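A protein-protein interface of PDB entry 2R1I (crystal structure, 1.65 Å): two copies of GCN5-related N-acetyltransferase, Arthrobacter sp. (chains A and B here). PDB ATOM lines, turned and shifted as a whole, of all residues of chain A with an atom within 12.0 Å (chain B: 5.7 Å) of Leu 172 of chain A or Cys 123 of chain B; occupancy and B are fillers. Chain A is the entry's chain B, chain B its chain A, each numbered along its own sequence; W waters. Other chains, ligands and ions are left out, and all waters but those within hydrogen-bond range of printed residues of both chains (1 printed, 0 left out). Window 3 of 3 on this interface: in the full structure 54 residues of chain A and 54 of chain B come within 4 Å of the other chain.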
ATOM      1  N   TYR A 167      17.838  35.242  19.797  1.00  0.00           N
ATOM      2  CA  TYR A 167      18.470  34.132  20.483  1.00  0.00           C
ATOM      3  C   TYR A 167      19.984  34.363  20.616  1.00  0.00           C
ATOM      4  O   TYR A 167      20.667  34.668  19.635  1.00  0.00           O
ATOM      5  CB  TYR A 167      18.179  32.854  19.702  1.00  0.00           C
ATOM      6  CG  TYR A 167      18.964  31.634  20.133  1.00  0.00           C
ATOM      7  CD1 TYR A 167      20.182  31.328  19.536  1.00  0.00           C
ATOM      8  CD2 TYR A 167      18.476  30.782  21.105  1.00  0.00           C
ATOM      9  CE1 TYR A 167      20.909  30.184  19.902  1.00  0.00           C
ATOM     10  CE2 TYR A 167      19.186  29.646  21.463  1.00  0.00           C
ATOM     11  CZ  TYR A 167      20.391  29.337  20.863  1.00  0.00           C
ATOM     12  OH  TYR A 167      21.105  28.210  21.240  1.00  0.00           O
ATOM     13  N   TYR A 168      20.470  34.289  21.857  1.00  0.00           N
ATOM     14  CA  TYR A 168      21.881  34.357  22.234  1.00  0.00           C
ATOM     15  C   TYR A 168      22.345  33.041  22.875  1.00  0.00           C
ATOM     16  O   TYR A 168      21.565  32.334  23.560  1.00  0.00           O
ATOM     17  CB  TYR A 168      22.102  35.511  23.239  1.00  0.00           C
ATOM     18  CG  TYR A 168      22.191  36.884  22.623  1.00  0.00           C
ATOM     19  CD1 TYR A 168      21.028  37.633  22.358  1.00  0.00           C
ATOM     20  CD2 TYR A 168      23.414  37.477  22.377  1.00  0.00           C
ATOM     21  CE1 TYR A 168      21.100  38.929  21.779  1.00  0.00           C
ATOM     22  CE2 TYR A 168      23.493  38.758  21.835  1.00  0.00           C
ATOM     23  CZ  TYR A 168      22.328  39.481  21.556  1.00  0.00           C
ATOM     24  OH  TYR A 168      22.441  40.731  20.974  1.00  0.00           O
ATOM     25  N   TYR A 169      23.602  32.679  22.629  1.00  0.00           N
ATOM     26  CA  TYR A 169      24.160  31.494  23.278  1.00  0.00           C
ATOM     27  C   TYR A 169      25.624  31.727  23.621  1.00  0.00           C
ATOM     28  O   TYR A 169      26.285  32.611  23.068  1.00  0.00           O
ATOM     29  CB  TYR A 169      24.042  30.252  22.393  1.00  0.00           C
ATOM     30  CG  TYR A 169      24.917  30.273  21.206  1.00  0.00           C
ATOM     31  CD1 TYR A 169      24.593  31.028  20.092  1.00  0.00           C
ATOM     32  CD2 TYR A 169      26.121  29.576  21.211  1.00  0.00           C
ATOM     33  CE1 TYR A 169      25.457  31.074  18.981  1.00  0.00           C
ATOM     34  CE2 TYR A 169      26.963  29.612  20.109  1.00  0.00           C
ATOM     35  CZ  TYR A 169      26.619  30.367  19.011  1.00  0.00           C
ATOM     36  OH  TYR A 169      27.464  30.388  17.915  1.00  0.00           O
ATOM     37  N   ARG A 170      26.090  30.917  24.566  1.00  0.00           N
ATOM     38  CA  ARG A 170      27.481  30.867  24.983  1.00  0.00           C
ATOM     39  C   ARG A 170      27.827  29.385  25.172  1.00  0.00           C
ATOM     40  O   ARG A 170      27.140  28.661  25.962  1.00  0.00           O
ATOM     41  CB  ARG A 170      27.734  31.688  26.270  1.00  0.00           C
ATOM     42  CG  ARG A 170      29.142  31.620  26.846  1.00  0.00           C
ATOM     43  CD  ARG A 170      29.258  32.586  28.033  1.00  0.00           C
ATOM     44  NE  ARG A 170      30.373  32.226  28.921  1.00  0.00           N
ATOM     45  CZ  ARG A 170      30.624  32.810  30.081  1.00  0.00           C
ATOM     46  NH1 ARG A 170      29.874  33.848  30.522  1.00  0.00           N
ATOM     47  NH2 ARG A 170      31.621  32.346  30.818  1.00  0.00           N
ATOM     48  N   GLU A 171      28.872  28.946  24.460  1.00  0.00           N
ATOM     49  CA  GLU A 171      29.404  27.599  24.639  1.00  0.00           C
ATOM     50  C   GLU A 171      30.260  27.619  25.900  1.00  0.00           C
ATOM     51  O   GLU A 171      31.059  28.548  26.107  1.00  0.00           O
ATOM     52  CB  GLU A 171      30.244  27.179  23.426  1.00  0.00           C
ATOM     53  CG  GLU A 171      29.408  27.040  22.174  1.00  0.00           C
ATOM     54  CD  GLU A 171      30.231  26.819  20.893  1.00  0.00           C
ATOM     55  OE1 GLU A 171      31.480  26.671  20.962  1.00  0.00           O
ATOM     56  OE2 GLU A 171      29.616  26.815  19.813  1.00  0.00           O
ATOM     57  N   LEU A 172      30.155  26.563  26.688  1.00  0.00           N
ATOM     58  CA  LEU A 172      30.807  26.429  27.992  1.00  0.00           C
ATOM     59  C   LEU A 172      31.676  25.176  28.002  1.00  0.00           C
ATOM     60  O   LEU A 172      31.502  24.282  27.146  1.00  0.00           O
ATOM     61  CB  LEU A 172      29.742  26.303  29.100  1.00  0.00           C
ATOM     62  CG  LEU A 172      28.854  27.535  29.311  1.00  0.00           C
ATOM     63  CD1 LEU A 172      27.774  27.270  30.424  1.00  0.00           C
ATOM     64  CD2 LEU A 172      29.694  28.801  29.614  1.00  0.00           C
ATOM     65  OXT LEU A 172      32.532  25.056  28.891  1.00  0.00           O
ATOM     66  N   LEU B 118      26.163  37.048  39.042  1.00  0.00           N
ATOM     67  CA  LEU B 118      25.132  36.026  38.883  1.00  0.00           C
ATOM     68  C   LEU B 118      25.367  35.231  37.588  1.00  0.00           C
ATOM     69  O   LEU B 118      25.176  33.999  37.566  1.00  0.00           O
ATOM     70  CB  LEU B 118      23.762  36.683  38.928  1.00  0.00           C
ATOM     71  CG  LEU B 118      23.258  36.982  40.349  1.00  0.00           C
ATOM     72  CD1 LEU B 118      22.125  37.996  40.344  1.00  0.00           C
ATOM     73  CD2 LEU B 118      22.804  35.648  41.050  1.00  0.00           C
ATOM     74  N   LEU B 119      25.748  35.941  36.519  1.00  0.00           N
ATOM     75  CA  LEU B 119      26.001  35.277  35.230  1.00  0.00           C
ATOM     76  C   LEU B 119      27.178  34.290  35.333  1.00  0.00           C
ATOM     77  O   LEU B 119      27.122  33.162  34.866  1.00  0.00           O
ATOM     78  CB  LEU B 119      26.181  36.288  34.085  1.00  0.00           C
ATOM     79  CG  LEU B 119      26.523  35.651  32.724  1.00  0.00           C
ATOM     80  CD1 LEU B 119      25.381  34.662  32.334  1.00  0.00           C
ATOM     81  CD2 LEU B 119      26.760  36.699  31.648  1.00  0.00           C
ATOM     82  N   ALA B 120      28.262  34.733  35.958  1.00  0.00           N
ATOM     83  CA  ALA B 120      29.419  33.882  36.142  1.00  0.00           C
ATOM     84  C   ALA B 120      29.100  32.646  36.982  1.00  0.00           C
ATOM     85  O   ALA B 120      29.520  31.522  36.656  1.00  0.00           O
ATOM     86  CB  ALA B 120      30.604  34.730  36.740  1.00  0.00           C
ATOM     87  N   ALA B 121      28.339  32.823  38.058  1.00  0.00           N
ATOM     88  CA  ALA B 121      27.939  31.693  38.885  1.00  0.00           C
ATOM     89  C   ALA B 121      27.047  30.709  38.083  1.00  0.00           C
ATOM     90  O   ALA B 121      27.169  29.488  38.239  1.00  0.00           O
ATOM     91  CB  ALA B 121      27.213  32.195  40.151  1.00  0.00           C
ATOM     92  N   SER B 122      26.169  31.252  37.233  1.00  0.00           N
ATOM     93  CA  SER B 122      25.284  30.432  36.349  1.00  0.00           C
ATOM     94  C   SER B 122      26.110  29.584  35.388  1.00  0.00           C
ATOM     95  O   SER B 122      25.883  28.405  35.251  1.00  0.00           O
ATOM     96  CB  SER B 122      24.327  31.323  35.553  1.00  0.00           C
ATOM     97  OG  SER B 122      23.464  32.095  36.413  1.00  0.00           O
ATOM     98  N   CYS B 123      27.145  30.161  34.774  1.00  0.00           N
ATOM     99  CA  CYS B 123      27.969  29.371  33.876  1.00  0.00           C
ATOM    100  C   CYS B 123      28.657  28.208  34.606  1.00  0.00           C
ATOM    101  O   CYS B 123      28.722  27.097  34.093  1.00  0.00           O
ATOM    102  CB  CYS B 123      28.988  30.250  33.175  1.00  0.00           C
ATOM    103  SG  CYS B 123      28.290  31.416  32.044  1.00  0.00           S
ATOM    104  N   GLY B 124      29.167  28.469  35.809  1.00  0.00           N
ATOM    105  CA  GLY B 124      29.774  27.439  36.634  1.00  0.00           C
ATOM    106  C   GLY B 124      28.836  26.308  37.000  1.00  0.00           C
ATOM    107  O   GLY B 124      29.185  25.142  36.944  1.00  0.00           O
ATOM    108  N   LEU B 125      27.630  26.676  37.381  1.00  0.00           N
ATOM    109  CA  LEU B 125      26.632  25.689  37.718  1.00  0.00           C
ATOM    110  C   LEU B 125      26.249  24.827  36.506  1.00  0.00           C
ATOM    111  O   LEU B 125      26.151  23.627  36.633  1.00  0.00           O
ATOM    112  CB  LEU B 125      25.432  26.372  38.346  1.00  0.00           C
ATOM    113  CG  LEU B 125      24.459  25.449  39.072  1.00  0.00           C
ATOM    114  CD1 LEU B 125      24.015  26.050  40.376  1.00  0.00           C
ATOM    115  CD2 LEU B 125      23.311  25.210  38.148  1.00  0.00           C
ATOM    116  N   VAL B 126      26.080  25.439  35.336  1.00  0.00           N
ATOM    117  CA  VAL B 126      25.812  24.693  34.106  1.00  0.00           C
ATOM    118  C   VAL B 126      26.926  23.687  33.795  1.00  0.00           C
ATOM    119  O   VAL B 126      26.656  22.504  33.523  1.00  0.00           O
ATOM    120  CB  VAL B 126      25.504  25.656  32.902  1.00  0.00           C
ATOM    121  CG1 VAL B 126      25.368  24.859  31.582  1.00  0.00           C
ATOM    122  CG2 VAL B 126      24.255  26.531  33.190  1.00  0.00           C
ATOM    123  N   ARG B 127      28.182  24.151  33.860  1.00  0.00           N
ATOM    124  CA  ARG B 127      29.327  23.261  33.659  1.00  0.00           C
ATOM    125  C   ARG B 127      29.292  22.091  34.644  1.00  0.00           C
ATOM    126  O   ARG B 127      29.570  20.952  34.255  1.00  0.00           O
ATOM    127  CB  ARG B 127      30.653  24.021  33.829  1.00  0.00           C
ATOM    128  CG  ARG B 127      31.156  24.729  32.567  1.00  0.00           C
ATOM    129  CD  ARG B 127      32.706  25.115  32.640  1.00  0.00           C
ATOM    130  NE  ARG B 127      33.017  26.155  31.650  1.00  0.00           N
ATOM    131  CZ  ARG B 127      32.951  27.472  31.878  1.00  0.00           C
ATOM    132  NH1 ARG B 127      32.613  27.955  33.086  1.00  0.00           N
ATOM    133  NH2 ARG B 127      33.255  28.328  30.892  1.00  0.00           N
ATOM    134  N   SER B 128      28.984  22.376  35.907  1.00  0.00           N
ATOM    135  CA  SER B 128      28.950  21.357  36.956  1.00  0.00           C
ATOM    136  C   SER B 128      27.941  20.277  36.660  1.00  0.00           C
ATOM    137  O   SER B 128      28.144  19.125  37.047  1.00  0.00           O
ATOM    138  CB  SER B 128      28.679  21.946  38.358  1.00  0.00           C
ATOM    139  OG  SER B 128      27.297  22.272  38.625  1.00  0.00           O
ATOM    140  N   GLY B 131      26.699  20.522  31.406  1.00  0.00           N
ATOM    141  CA  GLY B 131      26.236  21.329  30.282  1.00  0.00           C
ATOM    142  C   GLY B 131      27.331  22.120  29.581  1.00  0.00           C
ATOM    143  O   GLY B 131      28.339  22.565  30.191  1.00  0.00           O
ATOM    144  N   ALA B 132      27.172  22.226  28.270  1.00  0.00           N
ATOM    145  CA  ALA B 132      28.116  22.895  27.391  1.00  0.00           C
ATOM    146  C   ALA B 132      27.478  24.053  26.624  1.00  0.00           C
ATOM    147  O   ALA B 132      28.108  24.625  25.772  1.00  0.00           O
ATOM    148  CB  ALA B 132      28.743  21.878  26.399  1.00  0.00           C
ATOM    149  N   LEU B 133      26.226  24.396  26.960  1.00  0.00           N
ATOM    150  CA  LEU B 133      25.540  25.461  26.266  1.00  0.00           C
ATOM    151  C   LEU B 133      24.564  26.152  27.199  1.00  0.00           C
ATOM    152  O   LEU B 133      23.742  25.489  27.889  1.00  0.00           O
ATOM    153  CB  LEU B 133      24.776  24.927  25.077  1.00  0.00           C
ATOM    154  CG  LEU B 133      24.133  25.891  24.084  1.00  0.00           C
ATOM    155  CD1 LEU B 133      25.223  26.691  23.439  1.00  0.00           C
ATOM    156  CD2 LEU B 133      23.324  25.114  23.051  1.00  0.00           C
ATOM    157  N   LEU B 134      24.706  27.486  27.227  1.00  0.00           N
ATOM    158  CA  LEU B 134      23.755  28.379  27.923  1.00  0.00           C
ATOM    159  C   LEU B 134      23.107  29.341  26.931  1.00  0.00           C
ATOM    160  O   LEU B 134      23.830  30.050  26.171  1.00  0.00           O
ATOM    161  CB  LEU B 134      24.483  29.142  29.022  1.00  0.00           C
ATOM    162  CG  LEU B 134      23.637  30.077  29.909  1.00  0.00           C
ATOM    163  CD1 LEU B 134      22.497  29.311  30.560  1.00  0.00           C
ATOM    164  CD2 LEU B 134      24.591  30.770  30.956  1.00  0.00           C
ATOM    165  N   PHE B 154      28.501  35.899  25.052  1.00  0.00           N
ATOM    166  CA  PHE B 154      27.334  35.493  24.275  1.00  0.00           C
ATOM    167  C   PHE B 154      27.298  36.090  22.881  1.00  0.00           C
ATOM    168  O   PHE B 154      27.719  37.226  22.694  1.00  0.00           O
ATOM    169  CB  PHE B 154      26.030  35.860  24.994  1.00  0.00           C
ATOM    170  CG  PHE B 154      25.760  35.035  26.191  1.00  0.00           C
ATOM    171  CD1 PHE B 154      26.421  35.294  27.380  1.00  0.00           C
ATOM    172  CD2 PHE B 154      24.810  33.993  26.150  1.00  0.00           C
ATOM    173  CE1 PHE B 154      26.183  34.526  28.506  1.00  0.00           C
ATOM    174  CE2 PHE B 154      24.557  33.196  27.274  1.00  0.00           C
ATOM    175  CZ  PHE B 154      25.251  33.463  28.464  1.00  0.00           C
HETATM  176  O   HOH W   1      33.259  22.965  30.347  1.00  0.00           O
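No position is printed for both chains.
Among the printed residues, pairs that only touch across the chains: Tyr 169 of chain A with Leu 134 of chain B (3.3 Å), Tyr 169 of chain A with Phe 154 of chain B (3.3 Å), Glu 171 of chain A with Ala 132 of chain B (3.4 Å), Arg 170 of chain A with Leu 133 of chain B (3.6 Å), Leu 172 of chain A with Val 126 of chain B (3.6 Å), Arg 170 of chain A with Phe 154 of chain B (3.7 Å), Tyr 169 of chain A with Leu 133 of chain B (3.8 Å) and Leu 172 of chain A with Cys 123 of chain B (3.8 Å).
N of Gly 131 of chain B is in hydrogen-bond range of O of Val 126 of chain B (2.9 Å).
The backbone carbonyl oxygen (O) of Leu 119 of chain B is in hydrogen-bond range of the side-chain sulfur (SG) of Cys 123 of chain B.
Printed residues of chain A that touch a printed residue of chain B: Tyr 169, Arg 170, Glu 171 and Leu 172.
Hydrophobic or aromatic side chains of chain B that line the printed part of chain A: Val 126, Ala 132, Leu 133 and Phe 154.
Along chain B the printed residues that touch a printed residue of chain A span positions 123 to 154.
Among the printed residues, 12 pairs touch across the chains.
Water W1 bridges OXT of Leu 172 of chain A and NE of Arg 127 of chain B.
Of the printed residues of chain B, Leu 172 of chain A touches Cys 123, Val 126, Arg 127 and Ala 132.
Printed residues of chain A within 4 Å of Cys 123 of chain B: Arg 170 and Leu 172.
No residue of chain A comes within 4 Å of Leu 119 of chain B.
No residue of chain A comes within 4 Å of Ser 122 of chain B.
No residue of chain A comes within 4 Å of Gly 124 of chain B.
Of chain A, only Leu 172 comes within 4 Å of Val 126 of chain B.
Arg 127 of chain B touches just one residue of chain A: Leu 172 (3.0 Å).
No residue of chain A comes within 4 Å of Gly 131 of chain B.
Of the printed residues of chain A, Leu 133 of chain B touches Tyr 169 and Arg 170.
Printed residues of chain B within 4 Å of Tyr 169 of chain A: Leu 133, Leu 134 and Phe 154.
Printed residues of chain B within 4 Å of Glu 171 of chain A: Ala 132 (3.4 Å).
Printed residues of chain A within 4 Å of Phe 154 of chain B: Tyr 169 and Arg 170.
Leu 118 of chain B touches none of the printed residues of chain A.
Leu 125 of chain B touches none of the printed residues of chain A.
The nearest residue of chain B that does not touch Leu 172 of chain A is Leu 134 of chain B (4.04 Å).
The nearest residue of chain A that does not touch Cys 123 of chain B is Glu 171 of chain A (7.2 Å).
The nearest printed residue of chain B that does not touch Tyr 169 of chain A is Ala 132 of chain B (7.0 Å).
The side-chain sulfur (SG) of Cys 123 of chain B is in hydrogen-bond range of the guanidinium group (NH1) of Arg 170 of chain A, at 3.3 Å.
O of Ala 132 of chain B lies within hydrogen-bond range of N of Leu 172 of chain A (3.0 Å).
The chain-end carboxylate (OXT) of Leu 172 of chain A lies within salt-bridge range of the guanidinium group (NE) of Arg 127 of chain B (3.0 Å).
The backbone NH (N) of Arg 170 of chain A is in hydrogen-bond range of the backbone carbonyl oxygen (O) of Leu 134 of chain B.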
